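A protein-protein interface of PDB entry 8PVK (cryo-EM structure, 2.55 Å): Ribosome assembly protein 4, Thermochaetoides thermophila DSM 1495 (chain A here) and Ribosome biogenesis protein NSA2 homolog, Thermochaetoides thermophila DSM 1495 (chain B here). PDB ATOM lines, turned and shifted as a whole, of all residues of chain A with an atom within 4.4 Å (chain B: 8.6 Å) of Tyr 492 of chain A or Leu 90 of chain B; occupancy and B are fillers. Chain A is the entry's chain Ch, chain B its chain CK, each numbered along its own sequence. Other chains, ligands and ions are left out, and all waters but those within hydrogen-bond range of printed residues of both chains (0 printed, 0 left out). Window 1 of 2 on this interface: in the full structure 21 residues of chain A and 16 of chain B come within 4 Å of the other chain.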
ATOM      1  N   PRO A 148     -18.585  10.472   8.284  1.00  0.00           N
ATOM      2  CA  PRO A 148     -17.685  11.525   7.794  1.00  0.00           C
ATOM      3  C   PRO A 148     -18.315  12.911   7.767  1.00  0.00           C
ATOM      4  O   PRO A 148     -19.505  13.080   7.494  1.00  0.00           O
ATOM      5  CB  PRO A 148     -17.341  11.057   6.379  1.00  0.00           C
ATOM      6  CG  PRO A 148     -17.385   9.593   6.472  1.00  0.00           C
ATOM      7  CD  PRO A 148     -18.491   9.264   7.438  1.00  0.00           C
ATOM      8  N   ILE A 149     -17.485  13.907   8.067  1.00  0.00           N
ATOM      9  CA  ILE A 149     -17.901  15.304   8.056  1.00  0.00           C
ATOM     10  C   ILE A 149     -17.959  15.789   6.616  1.00  0.00           C
ATOM     11  O   ILE A 149     -16.992  15.643   5.860  1.00  0.00           O
ATOM     12  CB  ILE A 149     -16.936  16.163   8.886  1.00  0.00           C
ATOM     13  CG1 ILE A 149     -16.822  15.611  10.304  1.00  0.00           C
ATOM     14  CG2 ILE A 149     -17.390  17.614   8.907  1.00  0.00           C
ATOM     15  CD1 ILE A 149     -15.714  16.238  11.092  1.00  0.00           C
ATOM     16  N   LEU A 150     -19.092  16.376   6.233  1.00  0.00           N
ATOM     17  CA  LEU A 150     -19.282  16.831   4.866  1.00  0.00           C
ATOM     18  C   LEU A 150     -19.239  18.342   4.704  1.00  0.00           C
ATOM     19  O   LEU A 150     -19.023  18.814   3.583  1.00  0.00           O
ATOM     20  CB  LEU A 150     -20.614  16.305   4.313  1.00  0.00           C
ATOM     21  CG  LEU A 150     -20.862  14.812   4.545  1.00  0.00           C
ATOM     22  CD1 LEU A 150     -22.252  14.415   4.080  1.00  0.00           C
ATOM     23  CD2 LEU A 150     -19.801  13.974   3.851  1.00  0.00           C
ATOM     24  N   TRP A 424      -7.936  18.486  -9.533  1.00  0.00           N
ATOM     25  CA  TRP A 424      -7.729  17.052  -9.392  1.00  0.00           C
ATOM     26  C   TRP A 424      -6.385  16.603  -9.945  1.00  0.00           C
ATOM     27  O   TRP A 424      -6.078  15.408  -9.895  1.00  0.00           O
ATOM     28  CB  TRP A 424      -8.861  16.285 -10.078  1.00  0.00           C
ATOM     29  CG  TRP A 424     -10.167  16.326  -9.336  1.00  0.00           C
ATOM     30  CD1 TRP A 424     -10.843  17.436  -8.921  1.00  0.00           C
ATOM     31  CD2 TRP A 424     -10.959  15.203  -8.934  1.00  0.00           C
ATOM     32  NE1 TRP A 424     -12.001  17.075  -8.281  1.00  0.00           N
ATOM     33  CE2 TRP A 424     -12.096  15.709  -8.276  1.00  0.00           C
ATOM     34  CE3 TRP A 424     -10.815  13.818  -9.064  1.00  0.00           C
ATOM     35  CZ2 TRP A 424     -13.084  14.881  -7.751  1.00  0.00           C
ATOM     36  CZ3 TRP A 424     -11.795  12.999  -8.541  1.00  0.00           C
ATOM     37  CH2 TRP A 424     -12.915  13.532  -7.893  1.00  0.00           C
ATOM     38  N   TYR A 450      -9.140  18.969  -2.673  1.00  0.00           N
ATOM     39  CA  TYR A 450     -10.587  19.120  -2.628  1.00  0.00           C
ATOM     40  C   TYR A 450     -11.028  20.540  -2.305  1.00  0.00           C
ATOM     41  O   TYR A 450     -11.950  21.051  -2.951  1.00  0.00           O
ATOM     42  CB  TYR A 450     -11.190  18.140  -1.621  1.00  0.00           C
ATOM     43  CG  TYR A 450     -11.294  16.728  -2.148  1.00  0.00           C
ATOM     44  CD1 TYR A 450     -11.449  16.486  -3.507  1.00  0.00           C
ATOM     45  CD2 TYR A 450     -11.247  15.639  -1.290  1.00  0.00           C
ATOM     46  CE1 TYR A 450     -11.548  15.200  -3.996  1.00  0.00           C
ATOM     47  CE2 TYR A 450     -11.346  14.348  -1.770  1.00  0.00           C
ATOM     48  CZ  TYR A 450     -11.496  14.136  -3.123  1.00  0.00           C
ATOM     49  OH  TYR A 450     -11.595  12.852  -3.605  1.00  0.00           O
ATOM     50  N   GLN A 451     -10.408  21.206  -1.331  1.00  0.00           N
ATOM     51  CA  GLN A 451     -10.877  22.537  -0.966  1.00  0.00           C
ATOM     52  C   GLN A 451      -9.707  23.475  -0.714  1.00  0.00           C
ATOM     53  O   GLN A 451      -8.606  23.052  -0.358  1.00  0.00           O
ATOM     54  CB  GLN A 451     -11.789  22.501   0.266  1.00  0.00           C
ATOM     55  CG  GLN A 451     -13.227  22.127  -0.046  1.00  0.00           C
ATOM     56  CD  GLN A 451     -14.204  22.675   0.969  1.00  0.00           C
ATOM     57  OE1 GLN A 451     -13.822  23.396   1.889  1.00  0.00           O
ATOM     58  NE2 GLN A 451     -15.476  22.337   0.806  1.00  0.00           N
ATOM     59  N   GLU A 490      -9.494  11.066   4.193  1.00  0.00           N
ATOM     60  CA  GLU A 490      -9.598  12.188   3.267  1.00  0.00           C
ATOM     61  C   GLU A 490     -10.226  13.407   3.932  1.00  0.00           C
ATOM     62  O   GLU A 490     -11.075  13.286   4.818  1.00  0.00           O
ATOM     63  CB  GLU A 490     -10.422  11.793   2.043  1.00  0.00           C
ATOM     64  CG  GLU A 490      -9.973  10.510   1.372  1.00  0.00           C
ATOM     65  CD  GLU A 490     -10.764  10.207   0.118  1.00  0.00           C
ATOM     66  OE1 GLU A 490     -11.402  11.136  -0.422  1.00  0.00           O
ATOM     67  OE2 GLU A 490     -10.751   9.042  -0.330  1.00  0.00           O
ATOM     68  N   VAL A 491      -9.795  14.587   3.498  1.00  0.00           N
ATOM     69  CA  VAL A 491     -10.310  15.849   4.016  1.00  0.00           C
ATOM     70  C   VAL A 491     -11.384  16.354   3.060  1.00  0.00           C
ATOM     71  O   VAL A 491     -11.138  16.498   1.858  1.00  0.00           O
ATOM     72  CB  VAL A 491      -9.188  16.882   4.183  1.00  0.00           C
ATOM     73  CG1 VAL A 491      -9.759  18.211   4.636  1.00  0.00           C
ATOM     74  CG2 VAL A 491      -8.150  16.381   5.170  1.00  0.00           C
ATOM     75  N   TYR A 492     -12.572  16.626   3.595  1.00  0.00           N
ATOM     76  CA  TYR A 492     -13.706  17.038   2.779  1.00  0.00           C
ATOM     77  C   TYR A 492     -14.059  18.512   2.917  1.00  0.00           C
ATOM     78  O   TYR A 492     -14.545  19.109   1.952  1.00  0.00           O
ATOM     79  CB  TYR A 492     -14.939  16.199   3.125  1.00  0.00           C
ATOM     80  CG  TYR A 492     -14.876  14.774   2.623  1.00  0.00           C
ATOM     81  CD1 TYR A 492     -14.184  14.458   1.461  1.00  0.00           C
ATOM     82  CD2 TYR A 492     -15.523  13.749   3.301  1.00  0.00           C
ATOM     83  CE1 TYR A 492     -14.128  13.161   0.995  1.00  0.00           C
ATOM     84  CE2 TYR A 492     -15.472  12.447   2.841  1.00  0.00           C
ATOM     85  CZ  TYR A 492     -14.774  12.159   1.688  1.00  0.00           C
ATOM     86  OH  TYR A 492     -14.720  10.866   1.226  1.00  0.00           O
ATOM     87  N   ALA A 493     -13.836  19.116   4.083  1.00  0.00           N
ATOM     88  CA  ALA A 493     -14.241  20.494   4.322  1.00  0.00           C
ATOM     89  C   ALA A 493     -13.124  21.243   5.030  1.00  0.00           C
ATOM     90  O   ALA A 493     -12.561  20.741   6.007  1.00  0.00           O
ATOM     91  CB  ALA A 493     -15.527  20.550   5.153  1.00  0.00           C
ATOM     92  N   GLY A 506     -12.443  18.968   8.317  1.00  0.00           N
ATOM     93  CA  GLY A 506     -13.224  17.777   8.597  1.00  0.00           C
ATOM     94  C   GLY A 506     -13.254  16.884   7.382  1.00  0.00           C
ATOM     95  O   GLY A 506     -13.086  17.345   6.248  1.00  0.00           O
ATOM     96  N   GLY A 507     -13.468  15.596   7.616  1.00  0.00           N
ATOM     97  CA  GLY A 507     -13.521  14.667   6.510  1.00  0.00           C
ATOM     98  C   GLY A 507     -13.923  13.258   6.885  1.00  0.00           C
ATOM     99  O   GLY A 507     -14.778  13.051   7.750  1.00  0.00           O
ATOM    100  N   LYS A 508     -13.288  12.279   6.241  1.00  0.00           N
ATOM    101  CA  LYS A 508     -13.673  10.881   6.364  1.00  0.00           C
ATOM    102  C   LYS A 508     -13.257  10.254   7.692  1.00  0.00           C
ATOM    103  O   LYS A 508     -13.704   9.143   7.994  1.00  0.00           O
ATOM    104  CB  LYS A 508     -13.080  10.095   5.194  1.00  0.00           C
ATOM    105  CG  LYS A 508     -13.884   8.898   4.733  1.00  0.00           C
ATOM    106  CD  LYS A 508     -13.262   8.299   3.483  1.00  0.00           C
ATOM    107  CE  LYS A 508     -13.824   6.925   3.178  1.00  0.00           C
ATOM    108  NZ  LYS A 508     -13.100   6.278   2.050  1.00  0.00           N
ATOM    109  N   PRO B  82     -26.264   6.601  -2.447  1.00  0.00           N
ATOM    110  CA  PRO B  82     -24.971   5.945  -2.222  1.00  0.00           C
ATOM    111  C   PRO B  82     -24.877   5.304  -0.841  1.00  0.00           C
ATOM    112  O   PRO B  82     -25.845   5.333  -0.082  1.00  0.00           O
ATOM    113  CB  PRO B  82     -23.967   7.093  -2.360  1.00  0.00           C
ATOM    114  CG  PRO B  82     -24.649   8.083  -3.234  1.00  0.00           C
ATOM    115  CD  PRO B  82     -26.106   7.995  -2.894  1.00  0.00           C
ATOM    116  N   ASP B  84     -21.417   5.249   1.240  1.00  0.00           N
ATOM    117  CA  ASP B  84     -20.511   6.035   2.072  1.00  0.00           C
ATOM    118  C   ASP B  84     -20.855   7.516   1.964  1.00  0.00           C
ATOM    119  O   ASP B  84     -21.049   8.018   0.852  1.00  0.00           O
ATOM    120  CB  ASP B  84     -19.062   5.803   1.660  1.00  0.00           C
ATOM    121  CG  ASP B  84     -18.082   6.165   2.756  1.00  0.00           C
ATOM    122  OD1 ASP B  84     -17.906   5.357   3.692  1.00  0.00           O
ATOM    123  OD2 ASP B  84     -17.488   7.263   2.686  1.00  0.00           O
ATOM    124  N   PRO B  85     -20.958   8.233   3.083  1.00  0.00           N
ATOM    125  CA  PRO B  85     -21.245   9.676   3.030  1.00  0.00           C
ATOM    126  C   PRO B  85     -20.144  10.462   2.332  1.00  0.00           C
ATOM    127  O   PRO B  85     -18.986  10.457   2.753  1.00  0.00           O
ATOM    128  CB  PRO B  85     -21.369  10.061   4.508  1.00  0.00           C
ATOM    129  CG  PRO B  85     -21.780   8.804   5.180  1.00  0.00           C
ATOM    130  CD  PRO B  85     -21.064   7.706   4.453  1.00  0.00           C
ATOM    131  N   ILE B  86     -20.525  11.142   1.256  1.00  0.00           N
ATOM    132  CA  ILE B  86     -19.604  11.943   0.452  1.00  0.00           C
ATOM    133  C   ILE B  86     -20.185  13.345   0.330  1.00  0.00           C
ATOM    134  O   ILE B  86     -21.406  13.535   0.445  1.00  0.00           O
ATOM    135  CB  ILE B  86     -19.366  11.310  -0.941  1.00  0.00           C
ATOM    136  CG1 ILE B  86     -20.694  11.070  -1.659  1.00  0.00           C
ATOM    137  CG2 ILE B  86     -18.569  10.020  -0.816  1.00  0.00           C
ATOM    138  CD1 ILE B  86     -20.534  10.586  -3.078  1.00  0.00           C
ATOM    139  N   PRO B  87     -19.331  14.366   0.108  1.00  0.00           N
ATOM    140  CA  PRO B  87     -19.857  15.732  -0.041  1.00  0.00           C
ATOM    141  C   PRO B  87     -20.610  15.957  -1.343  1.00  0.00           C
ATOM    142  O   PRO B  87     -20.768  15.039  -2.154  1.00  0.00           O
ATOM    143  CB  PRO B  87     -18.598  16.609   0.021  1.00  0.00           C
ATOM    144  CG  PRO B  87     -17.535  15.745   0.560  1.00  0.00           C
ATOM    145  CD  PRO B  87     -17.859  14.357   0.156  1.00  0.00           C
ATOM    146  N   SER B  88     -21.079  17.192  -1.539  1.00  0.00           N
ATOM    147  CA  SER B  88     -21.883  17.515  -2.714  1.00  0.00           C
ATOM    148  C   SER B  88     -21.063  17.446  -3.996  1.00  0.00           C
ATOM    149  O   SER B  88     -21.557  16.986  -5.031  1.00  0.00           O
ATOM    150  CB  SER B  88     -22.509  18.899  -2.554  1.00  0.00           C
ATOM    151  OG  SER B  88     -23.436  18.919  -1.484  1.00  0.00           O
ATOM    152  N   TYR B  89     -19.807  17.899  -3.951  1.00  0.00           N
ATOM    153  CA  TYR B  89     -18.988  17.911  -5.157  1.00  0.00           C
ATOM    154  C   TYR B  89     -18.519  16.519  -5.562  1.00  0.00           C
ATOM    155  O   TYR B  89     -18.078  16.336  -6.701  1.00  0.00           O
ATOM    156  CB  TYR B  89     -17.788  18.845  -4.979  1.00  0.00           C
ATOM    157  CG  TYR B  89     -16.959  18.604  -3.735  1.00  0.00           C
ATOM    158  CD1 TYR B  89     -15.931  17.670  -3.730  1.00  0.00           C
ATOM    159  CD2 TYR B  89     -17.188  19.333  -2.575  1.00  0.00           C
ATOM    160  CE1 TYR B  89     -15.169  17.455  -2.601  1.00  0.00           C
ATOM    161  CE2 TYR B  89     -16.430  19.124  -1.441  1.00  0.00           C
ATOM    162  CZ  TYR B  89     -15.422  18.185  -1.460  1.00  0.00           C
ATOM    163  OH  TYR B  89     -14.662  17.973  -0.335  1.00  0.00           O
ATOM    164  N   LEU B  90     -18.596  15.540  -4.661  1.00  0.00           N
ATOM    165  CA  LEU B  90     -18.302  14.155  -5.000  1.00  0.00           C
ATOM    166  C   LEU B  90     -19.542  13.359  -5.378  1.00  0.00           C
ATOM    167  O   LEU B  90     -19.411  12.208  -5.806  1.00  0.00           O
ATOM    168  CB  LEU B  90     -17.589  13.460  -3.835  1.00  0.00           C
ATOM    169  CG  LEU B  90     -16.127  13.840  -3.604  1.00  0.00           C
ATOM    170  CD1 LEU B  90     -15.524  12.987  -2.503  1.00  0.00           C
ATOM    171  CD2 LEU B  90     -15.326  13.706  -4.887  1.00  0.00           C
ATOM    172  N   LEU B  91     -20.732  13.939  -5.233  1.00  0.00           N
ATOM    173  CA  LEU B  91     -21.958  13.252  -5.606  1.00  0.00           C
ATOM    174  C   LEU B  91     -22.074  13.142  -7.122  1.00  0.00           C
ATOM    175  O   LEU B  91     -21.490  13.933  -7.870  1.00  0.00           O
ATOM    176  CB  LEU B  91     -23.175  13.981  -5.040  1.00  0.00           C
ATOM    177  CG  LEU B  91     -23.587  13.606  -3.616  1.00  0.00           C
ATOM    178  CD1 LEU B  91     -24.690  14.523  -3.115  1.00  0.00           C
ATOM    179  CD2 LEU B  91     -24.024  12.153  -3.552  1.00  0.00           C
ATOM    180  N   ASP B  92     -22.813  12.122  -7.566  1.00  0.00           N
ATOM    181  CA  ASP B  92     -23.107  11.794  -8.962  1.00  0.00           C
ATOM    182  C   ASP B  92     -21.870  11.422  -9.771  1.00  0.00           C
ATOM    183  O   ASP B  92     -21.949  11.342 -11.003  1.00  0.00           O
ATOM    184  CB  ASP B  92     -23.857  12.924  -9.680  1.00  0.00           C
ATOM    185  CG  ASP B  92     -25.360  12.771  -9.597  1.00  0.00           C
ATOM    186  OD1 ASP B  92     -25.826  11.703  -9.149  1.00  0.00           O
ATOM    187  OD2 ASP B  92     -26.075  13.720  -9.980  1.00  0.00           O
ATOM    188  N   ARG B  93     -20.735  11.186  -9.124  1.00  0.00           N
ATOM    189  CA  ARG B  93     -19.526  10.739  -9.796  1.00  0.00           C
ATOM    190  C   ARG B  93     -19.356   9.233  -9.624  1.00  0.00           C
ATOM    191  O   ARG B  93     -20.054   8.584  -8.842  1.00  0.00           O
ATOM    192  CB  ARG B  93     -18.297  11.476  -9.255  1.00  0.00           C
ATOM    193  CG  ARG B  93     -18.386  12.987  -9.314  1.00  0.00           C
ATOM    194  CD  ARG B  93     -17.067  13.611  -8.895  1.00  0.00           C
ATOM    195  NE  ARG B  93     -17.046  15.055  -9.093  1.00  0.00           N
ATOM    196  CZ  ARG B  93     -16.736  15.650 -10.236  1.00  0.00           C
ATOM    197  NH1 ARG B  93     -16.417  14.951 -11.314  1.00  0.00           N
ATOM    198  NH2 ARG B  93     -16.745  16.977 -10.300  1.00  0.00           N
ATOM    199  N   ALA B  94     -18.406   8.680 -10.372  1.00  0.00           N
ATOM    200  CA  ALA B  94     -18.091   7.256 -10.292  1.00  0.00           C
ATOM    201  C   ALA B  94     -17.118   7.043  -9.141  1.00  0.00           C
ATOM    202  O   ALA B  94     -15.915   7.280  -9.275  1.00  0.00           O
ATOM    203  CB  ALA B  94     -17.514   6.757 -11.611  1.00  0.00           C
ATOM    204  N   ASN B  95     -17.638   6.594  -8.002  1.00  0.00           N
ATOM    205  CA  ASN B  95     -16.828   6.357  -6.821  1.00  0.00           C
ATOM    206  C   ASN B  95     -16.673   4.860  -6.569  1.00  0.00           C
ATOM    207  O   ASN B  95     -17.575   4.078  -6.885  1.00  0.00           O
ATOM    208  CB  ASN B  95     -17.452   7.019  -5.585  1.00  0.00           C
ATOM    209  CG  ASN B  95     -17.498   8.532  -5.695  1.00  0.00           C
ATOM    210  OD1 ASN B  95     -18.554   9.144  -5.535  1.00  0.00           O
ATOM    211  ND2 ASN B  95     -16.350   9.141  -5.966  1.00  0.00           N
ATOM    212  N   PRO B  96     -15.534   4.429  -6.024  1.00  0.00           N
ATOM    213  CA  PRO B  96     -15.352   3.004  -5.726  1.00  0.00           C
ATOM    214  C   PRO B  96     -16.282   2.529  -4.621  1.00  0.00           C
ATOM    215  O   PRO B  96     -16.712   3.301  -3.759  1.00  0.00           O
ATOM    216  CB  PRO B  96     -13.884   2.916  -5.289  1.00  0.00           C
ATOM    217  CG  PRO B  96     -13.239   4.133  -5.863  1.00  0.00           C
ATOM    218  CD  PRO B  96     -14.292   5.195  -5.827  1.00  0.00           C
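The side-chain hydroxyl (OH) of Tyr 89 of chain B is in hydrogen-bond range of the backbone carbonyl oxygen (O) of Tyr 492 of chain A.
The side-chain amide oxygen (OD1) of Asn 95 of chain B sits close to the backbone carbonyl oxygen (O) of Leu 90 of chain B, at 3.2 Å. The guanidinium group of Arg 93 of chain B is in hydrogen-bond range of the backbone carbonyl oxygen of Tyr 89 of chain B (2.9 Å). N of Tyr 492 of chain A is in hydrogen-bond range of O of Gly 506 of chain A (2.8 Å). The backbone carbonyl oxygen of Glu 490 of chain A lies within hydrogen-bond range of the backbone NH of Lys 508 of chain A.
Among the printed residues, pairs that only touch across the chains: Tyr 492 of chain A with Pro 87 of chain B, Leu 150 of chain A with Ile 86 of chain B, Tyr 450 of chain A with Tyr 89 of chain B, Lys 508 of chain A with Asp 84 of chain B, Tyr 492 of chain A with Leu 90 of chain B, Leu 150 of chain A with Pro 85 of chain B, Leu 150 of chain A with Pro 87 of chain B and Trp 424 of chain A with Leu 90 of chain B.
Tyr 492 of chain A touches just these residues of chain B: Pro 87, Tyr 89 and Leu 90. Printed residues of chain A within 4 Å of Leu 90 of chain B: Trp 424 and Tyr 492. Printed residues of chain A within 4 Å of Tyr 89 of chain B: Tyr 450 and Tyr 492. Printed residues of chain B within 4 Å of Tyr 450 of chain A: Tyr 89. Of the printed residues of chain A, Pro 87 of chain B touches Leu 150 and Tyr 492. Printed residues of chain A within 4 Å of Pro 85 of chain B: Leu 150 (3.8 Å). Glu 490 of chain A touches none of the printed residues of chain B. The nearest residue of chain A that does not touch Leu 90 of chain B is Tyr 450 of chain A (4.04 Å).
Printed residues of chain A that touch a printed residue of chain B: Leu 150, Trp 424, Tyr 450, Tyr 492 and Lys 508. Hydrophobic or aromatic side chains of chain A within 4 Å of the printed part of chain B: Leu 150, Trp 424, Tyr 450 and Tyr 492. Along chain A the printed residues that touch a printed residue of chain B span positions 150 to 508. Of the 14 printed residues of chain B, 6 touch a printed residue of chain A. Among the printed residues, no Asp or Glu carboxylate lies within 4 Å of a Lys or Arg side-chain nitrogen of the other chain.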
